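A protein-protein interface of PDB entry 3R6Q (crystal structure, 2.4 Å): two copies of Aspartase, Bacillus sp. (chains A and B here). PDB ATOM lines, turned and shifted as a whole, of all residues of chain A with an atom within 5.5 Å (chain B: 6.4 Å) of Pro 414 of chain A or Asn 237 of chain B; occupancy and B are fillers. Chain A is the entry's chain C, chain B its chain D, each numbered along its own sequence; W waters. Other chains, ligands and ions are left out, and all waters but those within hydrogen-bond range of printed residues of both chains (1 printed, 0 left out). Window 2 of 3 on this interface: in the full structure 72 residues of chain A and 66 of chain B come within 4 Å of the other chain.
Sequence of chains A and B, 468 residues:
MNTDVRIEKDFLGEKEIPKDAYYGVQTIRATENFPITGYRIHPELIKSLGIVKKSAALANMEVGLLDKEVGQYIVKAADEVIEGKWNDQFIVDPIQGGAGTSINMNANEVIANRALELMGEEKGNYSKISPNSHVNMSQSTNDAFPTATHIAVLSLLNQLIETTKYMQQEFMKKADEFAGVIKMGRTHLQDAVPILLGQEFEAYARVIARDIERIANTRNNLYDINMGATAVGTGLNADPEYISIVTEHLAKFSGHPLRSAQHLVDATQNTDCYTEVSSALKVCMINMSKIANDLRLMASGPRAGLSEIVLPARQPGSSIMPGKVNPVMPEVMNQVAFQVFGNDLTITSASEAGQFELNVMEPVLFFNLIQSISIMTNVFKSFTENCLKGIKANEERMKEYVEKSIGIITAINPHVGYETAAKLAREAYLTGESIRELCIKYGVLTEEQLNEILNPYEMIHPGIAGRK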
ATOM      1  N   ILE A 409       2.183  15.106 -25.639  1.00  0.00           N
ATOM      2  CA  ILE A 409       1.862  14.564 -24.317  1.00  0.00           C
ATOM      3  C   ILE A 409       2.610  15.276 -23.188  1.00  0.00           C
ATOM      4  O   ILE A 409       2.178  15.223 -22.036  1.00  0.00           O
ATOM      5  CB  ILE A 409       2.054  12.991 -24.244  1.00  0.00           C
ATOM      6  CG1 ILE A 409       1.234  12.366 -23.100  1.00  0.00           C
ATOM      7  CG2 ILE A 409       3.534  12.590 -24.123  1.00  0.00           C
ATOM      8  CD1 ILE A 409      -0.266  12.366 -23.325  1.00  0.00           C
ATOM      9  N   THR A 410       3.715  15.948 -23.514  1.00  0.00           N
ATOM     10  CA  THR A 410       4.532  16.642 -22.499  1.00  0.00           C
ATOM     11  C   THR A 410       3.787  17.855 -21.922  1.00  0.00           C
ATOM     12  O   THR A 410       3.928  18.178 -20.738  1.00  0.00           O
ATOM     13  CB  THR A 410       5.941  17.034 -23.043  1.00  0.00           C
ATOM     14  OG1 THR A 410       6.573  15.880 -23.608  1.00  0.00           O
ATOM     15  CG2 THR A 410       6.831  17.563 -21.932  1.00  0.00           C
ATOM     16  N   ALA A 411       2.984  18.502 -22.761  1.00  0.00           N
ATOM     17  CA  ALA A 411       2.128  19.592 -22.325  1.00  0.00           C
ATOM     18  C   ALA A 411       0.964  19.037 -21.509  1.00  0.00           C
ATOM     19  O   ALA A 411       0.585  19.615 -20.492  1.00  0.00           O
ATOM     20  CB  ALA A 411       1.627  20.391 -23.516  1.00  0.00           C
ATOM     21  N   ILE A 412       0.431  17.898 -21.949  1.00  0.00           N
ATOM     22  CA  ILE A 412      -0.719  17.243 -21.315  1.00  0.00           C
ATOM     23  C   ILE A 412      -0.380  16.592 -19.964  1.00  0.00           C
ATOM     24  O   ILE A 412      -1.202  16.634 -19.042  1.00  0.00           O
ATOM     25  CB  ILE A 412      -1.381  16.222 -22.288  1.00  0.00           C
ATOM     26  CG1 ILE A 412      -2.085  16.965 -23.431  1.00  0.00           C
ATOM     27  CG2 ILE A 412      -2.362  15.294 -21.559  1.00  0.00           C
ATOM     28  CD1 ILE A 412      -2.191  16.183 -24.735  1.00  0.00           C
ATOM     29  N   ASN A 413       0.821  16.018 -19.844  1.00  0.00           N
ATOM     30  CA  ASN A 413       1.222  15.260 -18.640  1.00  0.00           C
ATOM     31  C   ASN A 413       0.864  15.855 -17.259  1.00  0.00           C
ATOM     32  O   ASN A 413       0.220  15.162 -16.469  1.00  0.00           O
ATOM     33  CB  ASN A 413       2.702  14.827 -18.681  1.00  0.00           C
ATOM     34  CG  ASN A 413       3.238  14.429 -17.293  1.00  0.00           C
ATOM     35  OD1 ASN A 413       3.944  15.203 -16.653  1.00  0.00           O
ATOM     36  ND2 ASN A 413       2.876  13.239 -16.820  1.00  0.00           N
ATOM     37  N   PRO A 414       1.271  17.117 -16.962  1.00  0.00           N
ATOM     38  CA  PRO A 414       0.998  17.667 -15.620  1.00  0.00           C
ATOM     39  C   PRO A 414      -0.483  17.937 -15.292  1.00  0.00           C
ATOM     40  O   PRO A 414      -0.818  18.157 -14.121  1.00  0.00           O
ATOM     41  CB  PRO A 414       1.804  18.974 -15.597  1.00  0.00           C
ATOM     42  CG  PRO A 414       1.926  19.363 -17.023  1.00  0.00           C
ATOM     43  CD  PRO A 414       2.035  18.075 -17.789  1.00  0.00           C
ATOM     44  N   HIS A 415      -1.350  17.924 -16.306  1.00  0.00           N
ATOM     45  CA  HIS A 415      -2.804  18.028 -16.107  1.00  0.00           C
ATOM     46  C   HIS A 415      -3.488  16.662 -16.045  1.00  0.00           C
ATOM     47  O   HIS A 415      -4.715  16.575 -16.046  1.00  0.00           O
ATOM     48  CB  HIS A 415      -3.449  18.858 -17.219  1.00  0.00           C
ATOM     49  CG  HIS A 415      -3.075  20.304 -17.191  1.00  0.00           C
ATOM     50  ND1 HIS A 415      -2.039  20.818 -17.939  1.00  0.00           N
ATOM     51  CD2 HIS A 415      -3.598  21.346 -16.504  1.00  0.00           C
ATOM     52  CE1 HIS A 415      -1.939  22.116 -17.716  1.00  0.00           C
ATOM     53  NE2 HIS A 415      -2.871  22.462 -16.846  1.00  0.00           N
ATOM     54  N   VAL A 416      -2.694  15.600 -15.991  1.00  0.00           N
ATOM     55  CA  VAL A 416      -3.213  14.240 -16.054  1.00  0.00           C
ATOM     56  C   VAL A 416      -2.429  13.341 -15.100  1.00  0.00           C
ATOM     57  O   VAL A 416      -3.005  12.507 -14.408  1.00  0.00           O
ATOM     58  CB  VAL A 416      -3.182  13.712 -17.521  1.00  0.00           C
ATOM     59  CG1 VAL A 416      -3.023  12.211 -17.580  1.00  0.00           C
ATOM     60  CG2 VAL A 416      -4.425  14.156 -18.282  1.00  0.00           C
ATOM     61  N   GLY A 417      -1.116  13.535 -15.050  1.00  0.00           N
ATOM     62  CA  GLY A 417      -0.254  12.765 -14.167  1.00  0.00           C
ATOM     63  C   GLY A 417       0.572  11.752 -14.931  1.00  0.00           C
ATOM     64  O   GLY A 417       0.126  11.207 -15.939  1.00  0.00           O
ATOM     65  N   HIS A 461       7.058  27.782 -24.190  1.00  0.00           N
ATOM     66  CA  HIS A 461       7.682  28.769 -23.304  1.00  0.00           C
ATOM     67  C   HIS A 461       7.702  28.318 -21.839  1.00  0.00           C
ATOM     68  O   HIS A 461       6.868  27.505 -21.435  1.00  0.00           O
ATOM     69  CB  HIS A 461       7.007  30.138 -23.471  1.00  0.00           C
ATOM     70  CG  HIS A 461       7.358  30.823 -24.758  1.00  0.00           C
ATOM     71  ND1 HIS A 461       6.493  30.889 -25.830  1.00  0.00           N
ATOM     72  CD2 HIS A 461       8.497  31.440 -25.155  1.00  0.00           C
ATOM     73  CE1 HIS A 461       7.077  31.538 -26.822  1.00  0.00           C
ATOM     74  NE2 HIS A 461       8.295  31.879 -26.440  1.00  0.00           N
ATOM     75  N   GLY A 463       7.034  28.048 -17.918  1.00  0.00           N
ATOM     76  CA  GLY A 463       5.848  28.326 -17.116  1.00  0.00           C
ATOM     77  C   GLY A 463       5.315  27.090 -16.419  1.00  0.00           C
ATOM     78  O   GLY A 463       4.980  26.097 -17.079  1.00  0.00           O
ATOM     79  N   ILE A 464       5.231  27.167 -15.085  1.00  0.00           N
ATOM     80  CA  ILE A 464       4.757  26.074 -14.209  1.00  0.00           C
ATOM     81  C   ILE A 464       3.366  25.544 -14.604  1.00  0.00           C
ATOM     82  O   ILE A 464       2.578  26.262 -15.233  1.00  0.00           O
ATOM     83  CB  ILE A 464       4.749  26.518 -12.697  1.00  0.00           C
ATOM     84  CG1 ILE A 464       6.161  26.849 -12.200  1.00  0.00           C
ATOM     85  CG2 ILE A 464       4.103  25.457 -11.780  1.00  0.00           C
ATOM     86  CD1 ILE A 464       6.192  27.487 -10.812  1.00  0.00           C
ATOM     87  N   ALA A 465       3.104  24.284 -14.235  1.00  0.00           N
ATOM     88  CA  ALA A 465       1.793  23.610 -14.320  1.00  0.00           C
ATOM     89  C   ALA A 465       0.610  24.477 -14.781  1.00  0.00           C
ATOM     90  O   ALA A 465       0.368  24.596 -15.985  1.00  0.00           O
ATOM     91  CB  ALA A 465       1.472  22.892 -12.981  1.00  0.00           C
ATOM     92  N   THR B 230      15.217  22.374 -21.341  1.00  0.00           N
ATOM     93  CA  THR B 230      14.593  21.050 -21.568  1.00  0.00           C
ATOM     94  C   THR B 230      14.939  20.465 -22.948  1.00  0.00           C
ATOM     95  O   THR B 230      15.928  20.853 -23.551  1.00  0.00           O
ATOM     96  CB  THR B 230      13.056  21.024 -21.285  1.00  0.00           C
ATOM     97  OG1 THR B 230      12.349  21.686 -22.340  1.00  0.00           O
ATOM     98  CG2 THR B 230      12.732  21.672 -19.928  1.00  0.00           C
ATOM     99  N   THR B 234      12.615  25.061 -25.547  1.00  0.00           N
ATOM    100  CA  THR B 234      11.365  25.758 -25.278  1.00  0.00           C
ATOM    101  C   THR B 234      11.063  25.920 -23.797  1.00  0.00           C
ATOM    102  O   THR B 234      10.300  26.797 -23.417  1.00  0.00           O
ATOM    103  CB  THR B 234      10.160  25.116 -25.993  1.00  0.00           C
ATOM    104  OG1 THR B 234      10.126  23.709 -25.728  1.00  0.00           O
ATOM    105  CG2 THR B 234      10.238  25.363 -27.495  1.00  0.00           C
ATOM    106  N   GLY B 235      11.667  25.084 -22.965  1.00  0.00           N
ATOM    107  CA  GLY B 235      11.429  25.127 -21.525  1.00  0.00           C
ATOM    108  C   GLY B 235      10.015  24.722 -21.144  1.00  0.00           C
ATOM    109  O   GLY B 235       9.441  25.288 -20.220  1.00  0.00           O
ATOM    110  N   LEU B 236       9.450  23.749 -21.862  1.00  0.00           N
ATOM    111  CA  LEU B 236       8.120  23.211 -21.560  1.00  0.00           C
ATOM    112  C   LEU B 236       8.096  22.590 -20.166  1.00  0.00           C
ATOM    113  O   LEU B 236       8.842  21.653 -19.891  1.00  0.00           O
ATOM    114  CB  LEU B 236       7.676  22.192 -22.622  1.00  0.00           C
ATOM    115  CG  LEU B 236       6.212  21.709 -22.553  1.00  0.00           C
ATOM    116  CD1 LEU B 236       5.194  22.859 -22.375  1.00  0.00           C
ATOM    117  CD2 LEU B 236       5.842  20.843 -23.742  1.00  0.00           C
ATOM    118  N   ASN B 237       7.250  23.145 -19.294  1.00  0.00           N
ATOM    119  CA  ASN B 237       7.085  22.698 -17.893  1.00  0.00           C
ATOM    120  C   ASN B 237       8.143  23.174 -16.890  1.00  0.00           C
ATOM    121  O   ASN B 237       7.955  23.014 -15.679  1.00  0.00           O
ATOM    122  CB  ASN B 237       6.907  21.175 -17.800  1.00  0.00           C
ATOM    123  CG  ASN B 237       5.612  20.704 -18.438  1.00  0.00           C
ATOM    124  OD1 ASN B 237       4.698  21.502 -18.687  1.00  0.00           O
ATOM    125  ND2 ASN B 237       5.526  19.403 -18.713  1.00  0.00           N
ATOM    126  N   ALA B 238       9.241  23.746 -17.388  1.00  0.00           N
ATOM    127  CA  ALA B 238      10.297  24.298 -16.537  1.00  0.00           C
ATOM    128  C   ALA B 238       9.810  25.478 -15.683  1.00  0.00           C
ATOM    129  O   ALA B 238       9.127  26.387 -16.181  1.00  0.00           O
ATOM    130  CB  ALA B 238      11.494  24.721 -17.387  1.00  0.00           C
ATOM    131  N   ASP B 239      10.160  25.451 -14.401  1.00  0.00           N
ATOM    132  CA  ASP B 239       9.872  26.559 -13.495  1.00  0.00           C
ATOM    133  C   ASP B 239      10.901  27.663 -13.759  1.00  0.00           C
ATOM    134  O   ASP B 239      12.089  27.430 -13.563  1.00  0.00           O
ATOM    135  CB  ASP B 239       9.949  26.062 -12.035  1.00  0.00           C
ATOM    136  CG  ASP B 239       9.612  27.138 -11.015  1.00  0.00           C
ATOM    137  OD1 ASP B 239       9.311  26.790  -9.849  1.00  0.00           O
ATOM    138  OD2 ASP B 239       9.645  28.333 -11.364  1.00  0.00           O
HETATM  139  O   HOH W   1       2.218  21.918 -19.895  1.00  0.00           O
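No position is printed for both chains.
Of the 8 pairs that touch across the chains among the printed residues, none has its exchanged pair printed and touching as well.
Of chain B, only Asn 237 (3.8 Å) comes within 4 Å of Pro 414 of chain A.
Asn 237 of chain B touches just these residues of chain A: Thr 410 and Pro 414.
Printed residues of chain B within 4 Å of Ile 464 of chain A: Asp 239 (3.3 Å).
Of the printed residues of chain B, Ala 411 of chain A touches Leu 236 (3.8 Å).
Ala 465 of chain A touches none of the printed residues of chain B.
The nearest residue of chain A that does not touch Asn 237 of chain B is Gly 463 of chain A (4.1 Å).
The side-chain amide nitrogen of Asn 237 of chain B sits at hydrogen-bond distance from the backbone carbonyl oxygen of Thr 410 of chain A.
The backbone carbonyl oxygen (O) of Thr 234 of chain B lies close to the backbone NH (N) of His 461 of chain A (3.5 Å).
N of Gly 463 of chain A lies within hydrogen-bond range of O of Ala 238 of chain B, 3.2 Å away.
Hydrophobic or aromatic side chains of chain B that line the printed part of chain A: Leu 236.
Of the 13 printed residues of chain A, 6 touch a printed residue of chain B.
Among the printed residues, 8 pairs touch across the chains.
Among the printed residues, pairs that only touch across the chains: Ile 464 of chain A with Asp 239 of chain B, His 461 of chain A with Gly 235 of chain B, Ala 411 of chain A with Leu 236 of chain B, Pro 414 of chain A with Asn 237 of chain B and Thr 410 of chain A with Leu 236 of chain B.
Water W1 bridges OD1 of Asn 237 of chain B (2.8 Å) and O of Ala 411 of chain A (2.9 Å).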
